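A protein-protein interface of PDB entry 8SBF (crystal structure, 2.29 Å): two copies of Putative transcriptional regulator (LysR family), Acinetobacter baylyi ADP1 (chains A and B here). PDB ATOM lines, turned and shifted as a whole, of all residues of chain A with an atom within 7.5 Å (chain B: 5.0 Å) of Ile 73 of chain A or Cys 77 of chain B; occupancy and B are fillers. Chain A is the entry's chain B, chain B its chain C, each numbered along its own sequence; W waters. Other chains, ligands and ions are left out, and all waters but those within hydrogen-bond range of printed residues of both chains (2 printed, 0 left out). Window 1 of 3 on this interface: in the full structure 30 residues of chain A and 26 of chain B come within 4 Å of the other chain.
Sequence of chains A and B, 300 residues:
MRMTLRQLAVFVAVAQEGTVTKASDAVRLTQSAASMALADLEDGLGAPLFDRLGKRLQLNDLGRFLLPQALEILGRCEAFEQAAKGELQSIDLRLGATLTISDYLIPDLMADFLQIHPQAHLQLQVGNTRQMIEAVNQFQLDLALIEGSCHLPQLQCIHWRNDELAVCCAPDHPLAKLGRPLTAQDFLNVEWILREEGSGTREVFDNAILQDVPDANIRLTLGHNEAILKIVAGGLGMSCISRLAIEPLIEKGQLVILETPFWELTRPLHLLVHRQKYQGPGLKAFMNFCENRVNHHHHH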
ATOM      1  N   MET A   1      -2.218   1.008  12.991  1.00  0.00           N
ATOM      2  CA  MET A   1      -2.975   1.479  14.186  1.00  0.00           C
ATOM      3  C   MET A   1      -2.275   2.668  14.833  1.00  0.00           C
ATOM      4  O   MET A   1      -1.200   2.520  15.415  1.00  0.00           O
ATOM      5  CB  MET A   1      -3.124   0.345  15.205  1.00  0.00           C
ATOM      6  CG  MET A   1      -4.051   0.661  16.372  1.00  0.00           C
ATOM      7  SD  MET A   1      -5.775   0.216  16.063  1.00  0.00           S
ATOM      8  CE  MET A   1      -5.631  -1.545  15.769  1.00  0.00           C
ATOM      9  N   MET A   3      -4.270   4.825  16.919  1.00  0.00           N
ATOM     10  CA  MET A   3      -5.001   5.116  18.143  1.00  0.00           C
ATOM     11  C   MET A   3      -4.459   4.275  19.293  1.00  0.00           C
ATOM     12  O   MET A   3      -3.976   3.155  19.102  1.00  0.00           O
ATOM     13  CB  MET A   3      -6.501   4.870  17.950  1.00  0.00           C
ATOM     14  CG  MET A   3      -7.041   3.546  18.464  1.00  0.00           C
ATOM     15  SD  MET A   3      -8.833   3.461  18.224  1.00  0.00           S
ATOM     16  CE  MET A   3      -9.159   1.738  18.582  1.00  0.00           C
ATOM     17  N   THR A   4      -4.542   4.833  20.496  1.00  0.00           N
ATOM     18  CA  THR A   4      -3.937   4.253  21.681  1.00  0.00           C
ATOM     19  C   THR A   4      -4.986   4.068  22.772  1.00  0.00           C
ATOM     20  O   THR A   4      -6.051   4.688  22.752  1.00  0.00           O
ATOM     21  CB  THR A   4      -2.802   5.141  22.210  1.00  0.00           C
ATOM     22  OG1 THR A   4      -3.341   6.395  22.650  1.00  0.00           O
ATOM     23  CG2 THR A   4      -1.770   5.397  21.121  1.00  0.00           C
ATOM     24  N   LEU A   5      -4.666   3.196  23.731  1.00  0.00           N
ATOM     25  CA  LEU A   5      -5.537   3.032  24.889  1.00  0.00           C
ATOM     26  C   LEU A   5      -5.663   4.336  25.663  1.00  0.00           C
ATOM     27  O   LEU A   5      -6.726   4.641  26.215  1.00  0.00           O
ATOM     28  CB  LEU A   5      -5.009   1.917  25.792  1.00  0.00           C
ATOM     29  CG  LEU A   5      -5.200   0.499  25.252  1.00  0.00           C
ATOM     30  CD1 LEU A   5      -4.362  -0.498  26.039  1.00  0.00           C
ATOM     31  CD2 LEU A   5      -6.675   0.106  25.293  1.00  0.00           C
ATOM     32  N   LEU A   8      -8.344   6.270  23.909  1.00  0.00           N
ATOM     33  CA  LEU A   8      -9.649   5.702  24.228  1.00  0.00           C
ATOM     34  C   LEU A   8     -10.081   6.081  25.640  1.00  0.00           C
ATOM     35  O   LEU A   8     -11.249   6.413  25.873  1.00  0.00           O
ATOM     36  CB  LEU A   8      -9.620   4.181  24.074  1.00  0.00           C
ATOM     37  CG  LEU A   8      -9.678   3.609  22.657  1.00  0.00           C
ATOM     38  CD1 LEU A   8      -9.713   2.085  22.708  1.00  0.00           C
ATOM     39  CD2 LEU A   8     -10.881   4.145  21.899  1.00  0.00           C
ATOM     40  N   LEU A  45      -9.394   9.295  13.236  1.00  0.00           N
ATOM     41  CA  LEU A  45     -10.682   8.733  12.854  1.00  0.00           C
ATOM     42  C   LEU A  45     -11.324   9.487  11.695  1.00  0.00           C
ATOM     43  O   LEU A  45     -12.186   8.927  11.009  1.00  0.00           O
ATOM     44  CB  LEU A  45     -11.632   8.730  14.053  1.00  0.00           C
ATOM     45  CG  LEU A  45     -11.227   7.873  15.253  1.00  0.00           C
ATOM     46  CD1 LEU A  45     -12.299   7.946  16.338  1.00  0.00           C
ATOM     47  CD2 LEU A  45     -10.978   6.427  14.845  1.00  0.00           C
ATOM     48  N   LEU A  66     -19.696   4.824  19.110  1.00  0.00           N
ATOM     49  CA  LEU A  66     -18.388   4.259  19.412  1.00  0.00           C
ATOM     50  C   LEU A  66     -18.106   4.136  20.904  1.00  0.00           C
ATOM     51  O   LEU A  66     -17.272   3.311  21.292  1.00  0.00           O
ATOM     52  CB  LEU A  66     -17.287   5.111  18.776  1.00  0.00           C
ATOM     53  CG  LEU A  66     -17.175   5.077  17.253  1.00  0.00           C
ATOM     54  CD1 LEU A  66     -16.095   6.044  16.793  1.00  0.00           C
ATOM     55  CD2 LEU A  66     -16.880   3.669  16.761  1.00  0.00           C
ATOM     56  N   LEU A  67     -18.762   4.934  21.744  1.00  0.00           N
ATOM     57  CA  LEU A  67     -18.476   4.896  23.178  1.00  0.00           C
ATOM     58  C   LEU A  67     -18.592   3.496  23.766  1.00  0.00           C
ATOM     59  O   LEU A  67     -17.677   3.080  24.494  1.00  0.00           O
ATOM     60  CB  LEU A  67     -19.404   5.874  23.911  1.00  0.00           C
ATOM     61  CG  LEU A  67     -19.238   5.935  25.431  1.00  0.00           C
ATOM     62  CD1 LEU A  67     -17.876   6.497  25.805  1.00  0.00           C
ATOM     63  CD2 LEU A  67     -20.347   6.758  26.061  1.00  0.00           C
ATOM     64  N   PRO A  68     -19.655   2.727  23.506  1.00  0.00           N
ATOM     65  CA  PRO A  68     -19.696   1.358  24.052  1.00  0.00           C
ATOM     66  C   PRO A  68     -18.512   0.510  23.618  1.00  0.00           C
ATOM     67  O   PRO A  68     -17.998  -0.287  24.412  1.00  0.00           O
ATOM     68  CB  PRO A  68     -21.023   0.801  23.516  1.00  0.00           C
ATOM     69  CG  PRO A  68     -21.848   2.007  23.198  1.00  0.00           C
ATOM     70  CD  PRO A  68     -20.873   3.056  22.743  1.00  0.00           C
ATOM     71  N   GLN A  69     -18.064   0.665  22.369  1.00  0.00           N
ATOM     72  CA  GLN A  69     -16.917  -0.107  21.898  1.00  0.00           C
ATOM     73  C   GLN A  69     -15.648   0.280  22.645  1.00  0.00           C
ATOM     74  O   GLN A  69     -14.828  -0.584  22.976  1.00  0.00           O
ATOM     75  CB  GLN A  69     -16.736   0.091  20.393  1.00  0.00           C
ATOM     76  CG  GLN A  69     -17.908  -0.398  19.558  1.00  0.00           C
ATOM     77  CD  GLN A  69     -17.631  -0.320  18.070  1.00  0.00           C
ATOM     78  OE1 GLN A  69     -16.484  -0.412  17.635  1.00  0.00           O
ATOM     79  NE2 GLN A  69     -18.682  -0.144  17.281  1.00  0.00           N
ATOM     80  N   ALA A  70     -15.465   1.575  22.915  1.00  0.00           N
ATOM     81  CA  ALA A  70     -14.299   2.010  23.676  1.00  0.00           C
ATOM     82  C   ALA A  70     -14.322   1.428  25.084  1.00  0.00           C
ATOM     83  O   ALA A  70     -13.306   0.925  25.578  1.00  0.00           O
ATOM     84  CB  ALA A  70     -14.248   3.538  23.726  1.00  0.00           C
ATOM     85  N   LEU A  71     -15.481   1.486  25.746  1.00  0.00           N
ATOM     86  CA  LEU A  71     -15.600   0.905  27.078  1.00  0.00           C
ATOM     87  C   LEU A  71     -15.252  -0.578  27.067  1.00  0.00           C
ATOM     88  O   LEU A  71     -14.594  -1.077  27.987  1.00  0.00           O
ATOM     89  CB  LEU A  71     -17.017   1.113  27.612  1.00  0.00           C
ATOM     90  CG  LEU A  71     -17.403   2.549  27.967  1.00  0.00           C
ATOM     91  CD1 LEU A  71     -18.914   2.680  28.060  1.00  0.00           C
ATOM     92  CD2 LEU A  71     -16.747   2.970  29.271  1.00  0.00           C
ATOM     93  N   GLU A  72     -15.681  -1.301  26.030  1.00  0.00           N
ATOM     94  CA  GLU A  72     -15.406  -2.731  25.971  1.00  0.00           C
ATOM     95  C   GLU A  72     -13.923  -2.998  25.737  1.00  0.00           C
ATOM     96  O   GLU A  72     -13.360  -3.942  26.303  1.00  0.00           O
ATOM     97  CB  GLU A  72     -16.249  -3.385  24.876  1.00  0.00           C
ATOM     98  CG  GLU A  72     -15.912  -4.850  24.642  1.00  0.00           C
ATOM     99  CD  GLU A  72     -17.126  -5.686  24.281  1.00  0.00           C
ATOM    100  OE1 GLU A  72     -18.216  -5.110  24.068  1.00  0.00           O
ATOM    101  OE2 GLU A  72     -16.988  -6.926  24.216  1.00  0.00           O
ATOM    102  N   ILE A  73     -13.275  -2.180  24.907  1.00  0.00           N
ATOM    103  CA  ILE A  73     -11.844  -2.348  24.671  1.00  0.00           C
ATOM    104  C   ILE A  73     -11.064  -2.138  25.963  1.00  0.00           C
ATOM    105  O   ILE A  73     -10.145  -2.902  26.283  1.00  0.00           O
ATOM    106  CB  ILE A  73     -11.369  -1.390  23.562  1.00  0.00           C
ATOM    107  CG1 ILE A  73     -11.906  -1.849  22.204  1.00  0.00           C
ATOM    108  CG2 ILE A  73      -9.853  -1.304  23.544  1.00  0.00           C
ATOM    109  CD1 ILE A  73     -11.885  -0.775  21.141  1.00  0.00           C
ATOM    110  N   LEU A  74     -11.424  -1.107  26.729  1.00  0.00           N
ATOM    111  CA  LEU A  74     -10.705  -0.822  27.965  1.00  0.00           C
ATOM    112  C   LEU A  74     -10.980  -1.882  29.025  1.00  0.00           C
ATOM    113  O   LEU A  74     -10.075  -2.267  29.773  1.00  0.00           O
ATOM    114  CB  LEU A  74     -11.090   0.566  28.476  1.00  0.00           C
ATOM    115  CG  LEU A  74     -10.703   1.706  27.532  1.00  0.00           C
ATOM    116  CD1 LEU A  74     -11.460   2.979  27.871  1.00  0.00           C
ATOM    117  CD2 LEU A  74      -9.199   1.945  27.584  1.00  0.00           C
ATOM    118  N   GLY A  75     -12.220  -2.365  29.103  1.00  0.00           N
ATOM    119  CA  GLY A  75     -12.527  -3.420  30.056  1.00  0.00           C
ATOM    120  C   GLY A  75     -11.766  -4.700  29.765  1.00  0.00           C
ATOM    121  O   GLY A  75     -11.214  -5.330  30.671  1.00  0.00           O
ATOM    122  N   ARG A  76     -11.730  -5.103  28.494  1.00  0.00           N
ATOM    123  CA  ARG A  76     -10.974  -6.293  28.122  1.00  0.00           C
ATOM    124  C   ARG A  76      -9.493  -6.135  28.437  1.00  0.00           C
ATOM    125  O   ARG A  76      -8.819  -7.122  28.759  1.00  0.00           O
ATOM    126  CB  ARG A  76     -11.175  -6.596  26.638  1.00  0.00           C
ATOM    127  CG  ARG A  76     -12.575  -7.080  26.303  1.00  0.00           C
ATOM    128  CD  ARG A  76     -12.776  -7.223  24.804  1.00  0.00           C
ATOM    129  NE  ARG A  76     -14.027  -7.902  24.492  1.00  0.00           N
ATOM    130  CZ  ARG A  76     -14.168  -9.220  24.426  1.00  0.00           C
ATOM    131  NH1 ARG A  76     -13.151 -10.037  24.650  1.00  0.00           N
ATOM    132  NH2 ARG A  76     -15.359  -9.731  24.127  1.00  0.00           N
ATOM    133  N   CYS A  77      -8.970  -4.910  28.352  1.00  0.00           N
ATOM    134  CA  CYS A  77      -7.589  -4.675  28.761  1.00  0.00           C
ATOM    135  C   CYS A  77      -7.431  -4.828  30.268  1.00  0.00           C
ATOM    136  O   CYS A  77      -6.446  -5.410  30.736  1.00  0.00           O
ATOM    137  CB  CYS A  77      -7.138  -3.287  28.307  1.00  0.00           C
ATOM    138  SG  CYS A  77      -6.843  -3.157  26.530  1.00  0.00           S
ATOM    139  N   GLU A  78      -8.387  -4.313  31.043  1.00  0.00           N
ATOM    140  CA  GLU A  78      -8.371  -4.556  32.481  1.00  0.00           C
ATOM    141  C   GLU A  78      -8.402  -6.048  32.778  1.00  0.00           C
ATOM    142  O   GLU A  78      -7.683  -6.530  33.661  1.00  0.00           O
ATOM    143  CB  GLU A  78      -9.554  -3.855  33.151  1.00  0.00           C
ATOM    144  CG  GLU A  78      -9.319  -2.380  33.428  1.00  0.00           C
ATOM    145  CD  GLU A  78     -10.542  -1.682  33.996  1.00  0.00           C
ATOM    146  OE1 GLU A  78     -11.668  -1.973  33.534  1.00  0.00           O
ATOM    147  OE2 GLU A  78     -10.377  -0.843  34.906  1.00  0.00           O
ATOM    148  N   ALA A  79      -9.226  -6.799  32.044  1.00  0.00           N
ATOM    149  CA  ALA A  79      -9.300  -8.238  32.262  1.00  0.00           C
ATOM    150  C   ALA A  79      -8.004  -8.924  31.847  1.00  0.00           C
ATOM    151  O   ALA A  79      -7.564  -9.878  32.498  1.00  0.00           O
ATOM    152  CB  ALA A  79     -10.489  -8.821  31.498  1.00  0.00           C
ATOM    153  N   TYR A 278     -19.985  -2.336  28.991  1.00  0.00           N
ATOM    154  CA  TYR A 278     -19.223  -3.543  29.279  1.00  0.00           C
ATOM    155  C   TYR A 278     -18.922  -3.627  30.771  1.00  0.00           C
ATOM    156  O   TYR A 278     -18.466  -2.656  31.383  1.00  0.00           O
ATOM    157  CB  TYR A 278     -17.927  -3.536  28.467  1.00  0.00           C
ATOM    158  CG  TYR A 278     -17.060  -4.765  28.631  1.00  0.00           C
ATOM    159  CD1 TYR A 278     -17.224  -5.869  27.806  1.00  0.00           C
ATOM    160  CD2 TYR A 278     -16.067  -4.814  29.600  1.00  0.00           C
ATOM    161  CE1 TYR A 278     -16.430  -6.992  27.948  1.00  0.00           C
ATOM    162  CE2 TYR A 278     -15.269  -5.931  29.751  1.00  0.00           C
ATOM    163  CZ  TYR A 278     -15.454  -7.017  28.922  1.00  0.00           C
ATOM    164  OH  TYR A 278     -14.660  -8.134  29.066  1.00  0.00           O
ATOM    165  N   LEU B   5      -1.451  -1.041  23.193  1.00  0.00           N
ATOM    166  CA  LEU B   5      -1.847  -1.813  22.020  1.00  0.00           C
ATOM    167  C   LEU B   5      -0.628  -2.322  21.262  1.00  0.00           C
ATOM    168  O   LEU B   5      -0.636  -3.440  20.734  1.00  0.00           O
ATOM    169  CB  LEU B   5      -2.731  -0.963  21.106  1.00  0.00           C
ATOM    170  CG  LEU B   5      -4.107  -0.595  21.662  1.00  0.00           C
ATOM    171  CD1 LEU B   5      -4.825   0.368  20.725  1.00  0.00           C
ATOM    172  CD2 LEU B   5      -4.951  -1.843  21.891  1.00  0.00           C
ATOM    173  N   GLU B  72      -8.745 -10.645  20.487  1.00  0.00           N
ATOM    174  CA  GLU B  72     -10.023  -9.942  20.549  1.00  0.00           C
ATOM    175  C   GLU B  72      -9.818  -8.442  20.723  1.00  0.00           C
ATOM    176  O   GLU B  72     -10.477  -7.641  20.052  1.00  0.00           O
ATOM    177  CB  GLU B  72     -10.871 -10.502  21.690  1.00  0.00           C
ATOM    178  CG  GLU B  72     -11.537 -11.833  21.377  1.00  0.00           C
ATOM    179  CD  GLU B  72     -12.848 -11.674  20.623  1.00  0.00           C
ATOM    180  OE1 GLU B  72     -13.155 -10.544  20.184  1.00  0.00           O
ATOM    181  OE2 GLU B  72     -13.577 -12.680  20.478  1.00  0.00           O
ATOM    182  N   ILE B  73      -8.907  -8.047  21.615  1.00  0.00           N
ATOM    183  CA  ILE B  73      -8.642  -6.625  21.827  1.00  0.00           C
ATOM    184  C   ILE B  73      -8.205  -5.969  20.524  1.00  0.00           C
ATOM    185  O   ILE B  73      -8.765  -4.951  20.102  1.00  0.00           O
ATOM    186  CB  ILE B  73      -7.589  -6.436  22.934  1.00  0.00           C
ATOM    187  CG1 ILE B  73      -8.181  -6.807  24.296  1.00  0.00           C
ATOM    188  CG2 ILE B  73      -7.074  -5.000  22.933  1.00  0.00           C
ATOM    189  CD1 ILE B  73      -7.158  -6.920  25.404  1.00  0.00           C
ATOM    190  N   LEU B  74      -7.194  -6.543  19.866  1.00  0.00           N
ATOM    191  CA  LEU B  74      -6.713  -5.969  18.612  1.00  0.00           C
ATOM    192  C   LEU B  74      -7.807  -5.972  17.552  1.00  0.00           C
ATOM    193  O   LEU B  74      -7.954  -5.001  16.801  1.00  0.00           O
ATOM    194  CB  LEU B  74      -5.490  -6.738  18.118  1.00  0.00           C
ATOM    195  CG  LEU B  74      -4.215  -6.610  18.952  1.00  0.00           C
ATOM    196  CD1 LEU B  74      -3.149  -7.559  18.428  1.00  0.00           C
ATOM    197  CD2 LEU B  74      -3.705  -5.181  18.941  1.00  0.00           C
ATOM    198  N   GLY B  75      -8.584  -7.052  17.476  1.00  0.00           N
ATOM    199  CA  GLY B  75      -9.643  -7.118  16.483  1.00  0.00           C
ATOM    200  C   GLY B  75     -10.696  -6.044  16.676  1.00  0.00           C
ATOM    201  O   GLY B  75     -11.219  -5.490  15.705  1.00  0.00           O
ATOM    202  N   ARG B  76     -11.017  -5.729  17.932  1.00  0.00           N
ATOM    203  CA  ARG B  76     -12.029  -4.715  18.209  1.00  0.00           C
ATOM    204  C   ARG B  76     -11.489  -3.304  18.025  1.00  0.00           C
ATOM    205  O   ARG B  76     -12.255  -2.395  17.686  1.00  0.00           O
ATOM    206  CB  ARG B  76     -12.575  -4.900  19.624  1.00  0.00           C
ATOM    207  CG  ARG B  76     -13.399  -6.165  19.767  1.00  0.00           C
ATOM    208  CD  ARG B  76     -13.758  -6.474  21.207  1.00  0.00           C
ATOM    209  NE  ARG B  76     -14.521  -7.714  21.286  1.00  0.00           N
ATOM    210  CZ  ARG B  76     -15.826  -7.805  21.069  1.00  0.00           C
ATOM    211  NH1 ARG B  76     -16.561  -6.736  20.806  1.00  0.00           N
ATOM    212  NH2 ARG B  76     -16.410  -8.999  21.112  1.00  0.00           N
ATOM    213  N   CYS B  77     -10.189  -3.100  18.240  1.00  0.00           N
ATOM    214  CA  CYS B  77      -9.590  -1.811  17.915  1.00  0.00           C
ATOM    215  C   CYS B  77      -9.638  -1.555  16.414  1.00  0.00           C
ATOM    216  O   CYS B  77      -9.880  -0.422  15.978  1.00  0.00           O
ATOM    217  CB  CYS B  77      -8.150  -1.752  18.426  1.00  0.00           C
ATOM    218  SG  CYS B  77      -8.003  -1.641  20.223  1.00  0.00           S
ATOM    219  N   GLU B  78      -9.414  -2.593  15.605  1.00  0.00           N
ATOM    220  CA  GLU B  78      -9.536  -2.439  14.159  1.00  0.00           C
ATOM    221  C   GLU B  78     -10.982  -2.182  13.754  1.00  0.00           C
ATOM    222  O   GLU B  78     -11.251  -1.348  12.881  1.00  0.00           O
ATOM    223  CB  GLU B  78      -8.987  -3.680  13.454  1.00  0.00           C
ATOM    224  CG  GLU B  78      -7.587  -3.495  12.890  1.00  0.00           C
ATOM    225  CD  GLU B  78      -6.754  -4.765  12.943  1.00  0.00           C
ATOM    226  OE1 GLU B  78      -7.334  -5.856  13.135  1.00  0.00           O
ATOM    227  OE2 GLU B  78      -5.516  -4.669  12.801  1.00  0.00           O
ATOM    228  N   ALA B  79     -11.930  -2.890  14.374  1.00  0.00           N
ATOM    229  CA  ALA B  79     -13.337  -2.607  14.121  1.00  0.00           C
ATOM    230  C   ALA B  79     -13.687  -1.184  14.538  1.00  0.00           C
ATOM    231  O   ALA B  79     -14.440  -0.490  13.845  1.00  0.00           O
ATOM    232  CB  ALA B  79     -14.218  -3.613  14.862  1.00  0.00           C
ATOM    233  N   PHE B  80     -13.142  -0.735  15.671  1.00  0.00           N
ATOM    234  CA  PHE B  80     -13.378   0.630  16.133  1.00  0.00           C
ATOM    235  C   PHE B  80     -12.915   1.644  15.092  1.00  0.00           C
ATOM    236  O   PHE B  80     -13.650   2.576  14.745  1.00  0.00           O
ATOM    237  CB  PHE B  80     -12.654   0.843  17.468  1.00  0.00           C
ATOM    238  CG  PHE B  80     -12.954   2.161  18.129  1.00  0.00           C
ATOM    239  CD1 PHE B  80     -12.301   3.316  17.736  1.00  0.00           C
ATOM    240  CD2 PHE B  80     -13.874   2.236  19.162  1.00  0.00           C
ATOM    241  CE1 PHE B  80     -12.572   4.526  18.349  1.00  0.00           C
ATOM    242  CE2 PHE B  80     -14.145   3.444  19.779  1.00  0.00           C
ATOM    243  CZ  PHE B  80     -13.495   4.588  19.372  1.00  0.00           C
ATOM    244  N   GLU B  81     -11.693   1.473  14.579  1.00  0.00           N
ATOM    245  CA  GLU B  81     -11.171   2.416  13.594  1.00  0.00           C
ATOM    246  C   GLU B  81     -11.965   2.361  12.295  1.00  0.00           C
ATOM    247  O   GLU B  81     -12.294   3.403  11.718  1.00  0.00           O
ATOM    248  CB  GLU B  81      -9.691   2.139  13.326  1.00  0.00           C
ATOM    249  CG  GLU B  81      -8.747   2.714  14.370  1.00  0.00           C
ATOM    250  CD  GLU B  81      -7.309   2.781  13.883  1.00  0.00           C
ATOM    251  OE1 GLU B  81      -7.025   2.261  12.781  1.00  0.00           O
ATOM    252  OE2 GLU B  81      -6.464   3.359  14.599  1.00  0.00           O
HETATM  253  O   HOH W   1     -14.920  -2.508  18.501  1.00  0.00           O
HETATM  254  O   HOH W   2      -1.856   1.951  23.412  1.00  0.00           O
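The guanidinium group of Arg 76 of chain B is in salt-bridge range of the side-chain carboxylate of Glu 72 of chain A, at 3.4 Å.
The side-chain sulfur (SD) of Met 1 of chain A lies close to the side-chain carboxylate (OE2) of Glu 81 of chain B (3.5 Å).
NE of Arg 76 of chain B lies close to NE of Arg 76 of chain A (3.2 Å).
The guanidinium group (NE) of Arg 76 of chain B lies within salt-bridge range of the side-chain carboxylate (OE1) of Glu 72 of chain B.
The side-chain sulfur (SG) of Cys 77 of chain B sits at hydrogen-bond distance from the backbone carbonyl oxygen (O) of Ile 73 of chain B (3.4 Å).
The side-chain carboxylate (OE2) of Glu 72 of chain A is in salt-bridge range of the guanidinium group (NE) of Arg 76 of chain A (3.1 Å).
O of Ile 73 of chain A sits at hydrogen-bond distance from SG of Cys 77 of chain A, 3.3 Å away.
CB of Cys 77 of chain B touches CE of Met 1 of chain A (3.7 Å).
CE of Met 1 of chain A touches N of Glu 78 of chain B, 3.9 Å away.
OE2 of Glu 81 of chain B touches N of Met 3 of chain A, 3.5 Å away.
Leu 8 of chain A touches Phe 80 of chain B.
Leu 45 of chain A touches Phe 80 of chain B.
Phe 80 of chain B touches Leu 66 of chain A (CE2 to O, 3.5 Å).
CA of Phe 80 of chain B touches OE1 of Gln 69 of chain A, 3.6 Å away.
CE2 of Phe 80 of chain B touches N of Ala 70 of chain A, 3.9 Å away.
NH1 of Arg 76 of chain A touches CB of Glu 72 of chain B (3.8 Å).
Arg 76 of chain A touches Ile 73 of chain B (O to CD1, 3.7 Å).
Printed residues of chain B within 4 Å of Met 1 of chain A: Cys 77 (3.7 Å), Glu 78 (3.9 Å) and Glu 81 (3.5 Å).
Printed residues of chain B within 4 Å of Leu 66 of chain A: Phe 80 (3.5 Å).
Of chain B, only Arg 76 and Cys 77 come within 4 Å of Ile 73 of chain A.
Gly 75 of chain A touches none of the printed residues of chain B.
Gly 75 of chain B touches none of the printed residues of chain A.
Cys 77 of chain B touches just these residues of chain A: Met 1, Met 3 and Ile 73.
Hydrophobic or aromatic side chains of chain B within 4 Å of the printed part of chain A: Leu 5, Ile 73 and Phe 80.
Hydrophobic or aromatic side chains of chain A that line the printed part of chain B: Met 1, Met 3, Leu 5, Leu 8, Leu 45, Leu 66, Ala 70 and Ile 73.
Among the printed residues, 20 pairs touch across the chains.
Leu 5 of chain A touches its own counterpart, Leu 5 of chain B.
Glu 72 of chain A touches Arg 76 of chain B, and with the chains exchanged Arg 76 of chain A touches Glu 72 of chain B.
Ile 73 of chain A touches Arg 76 of chain B, and with the chains exchanged Arg 76 of chain A touches Ile 73 of chain B.
Ile 73 of chain A touches Cys 77 of chain B, and with the chains exchanged Cys 77 of chain A touches Ile 73 of chain B.
Positions printed for both chains: 5, 72, 73, 74, 75, 76, 77, 78 and 79.
Water W1 bridges the side-chain amide oxygen (OE1) of Gln 69 of chain A (2.8 Å) and the backbone carbonyl oxygen (O) of Arg 76 of chain B (2.8 Å).
Water W2 bridges N of Leu 5 of chain B (3.0 Å) and N of Leu 5 of chain A (3.1 Å).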
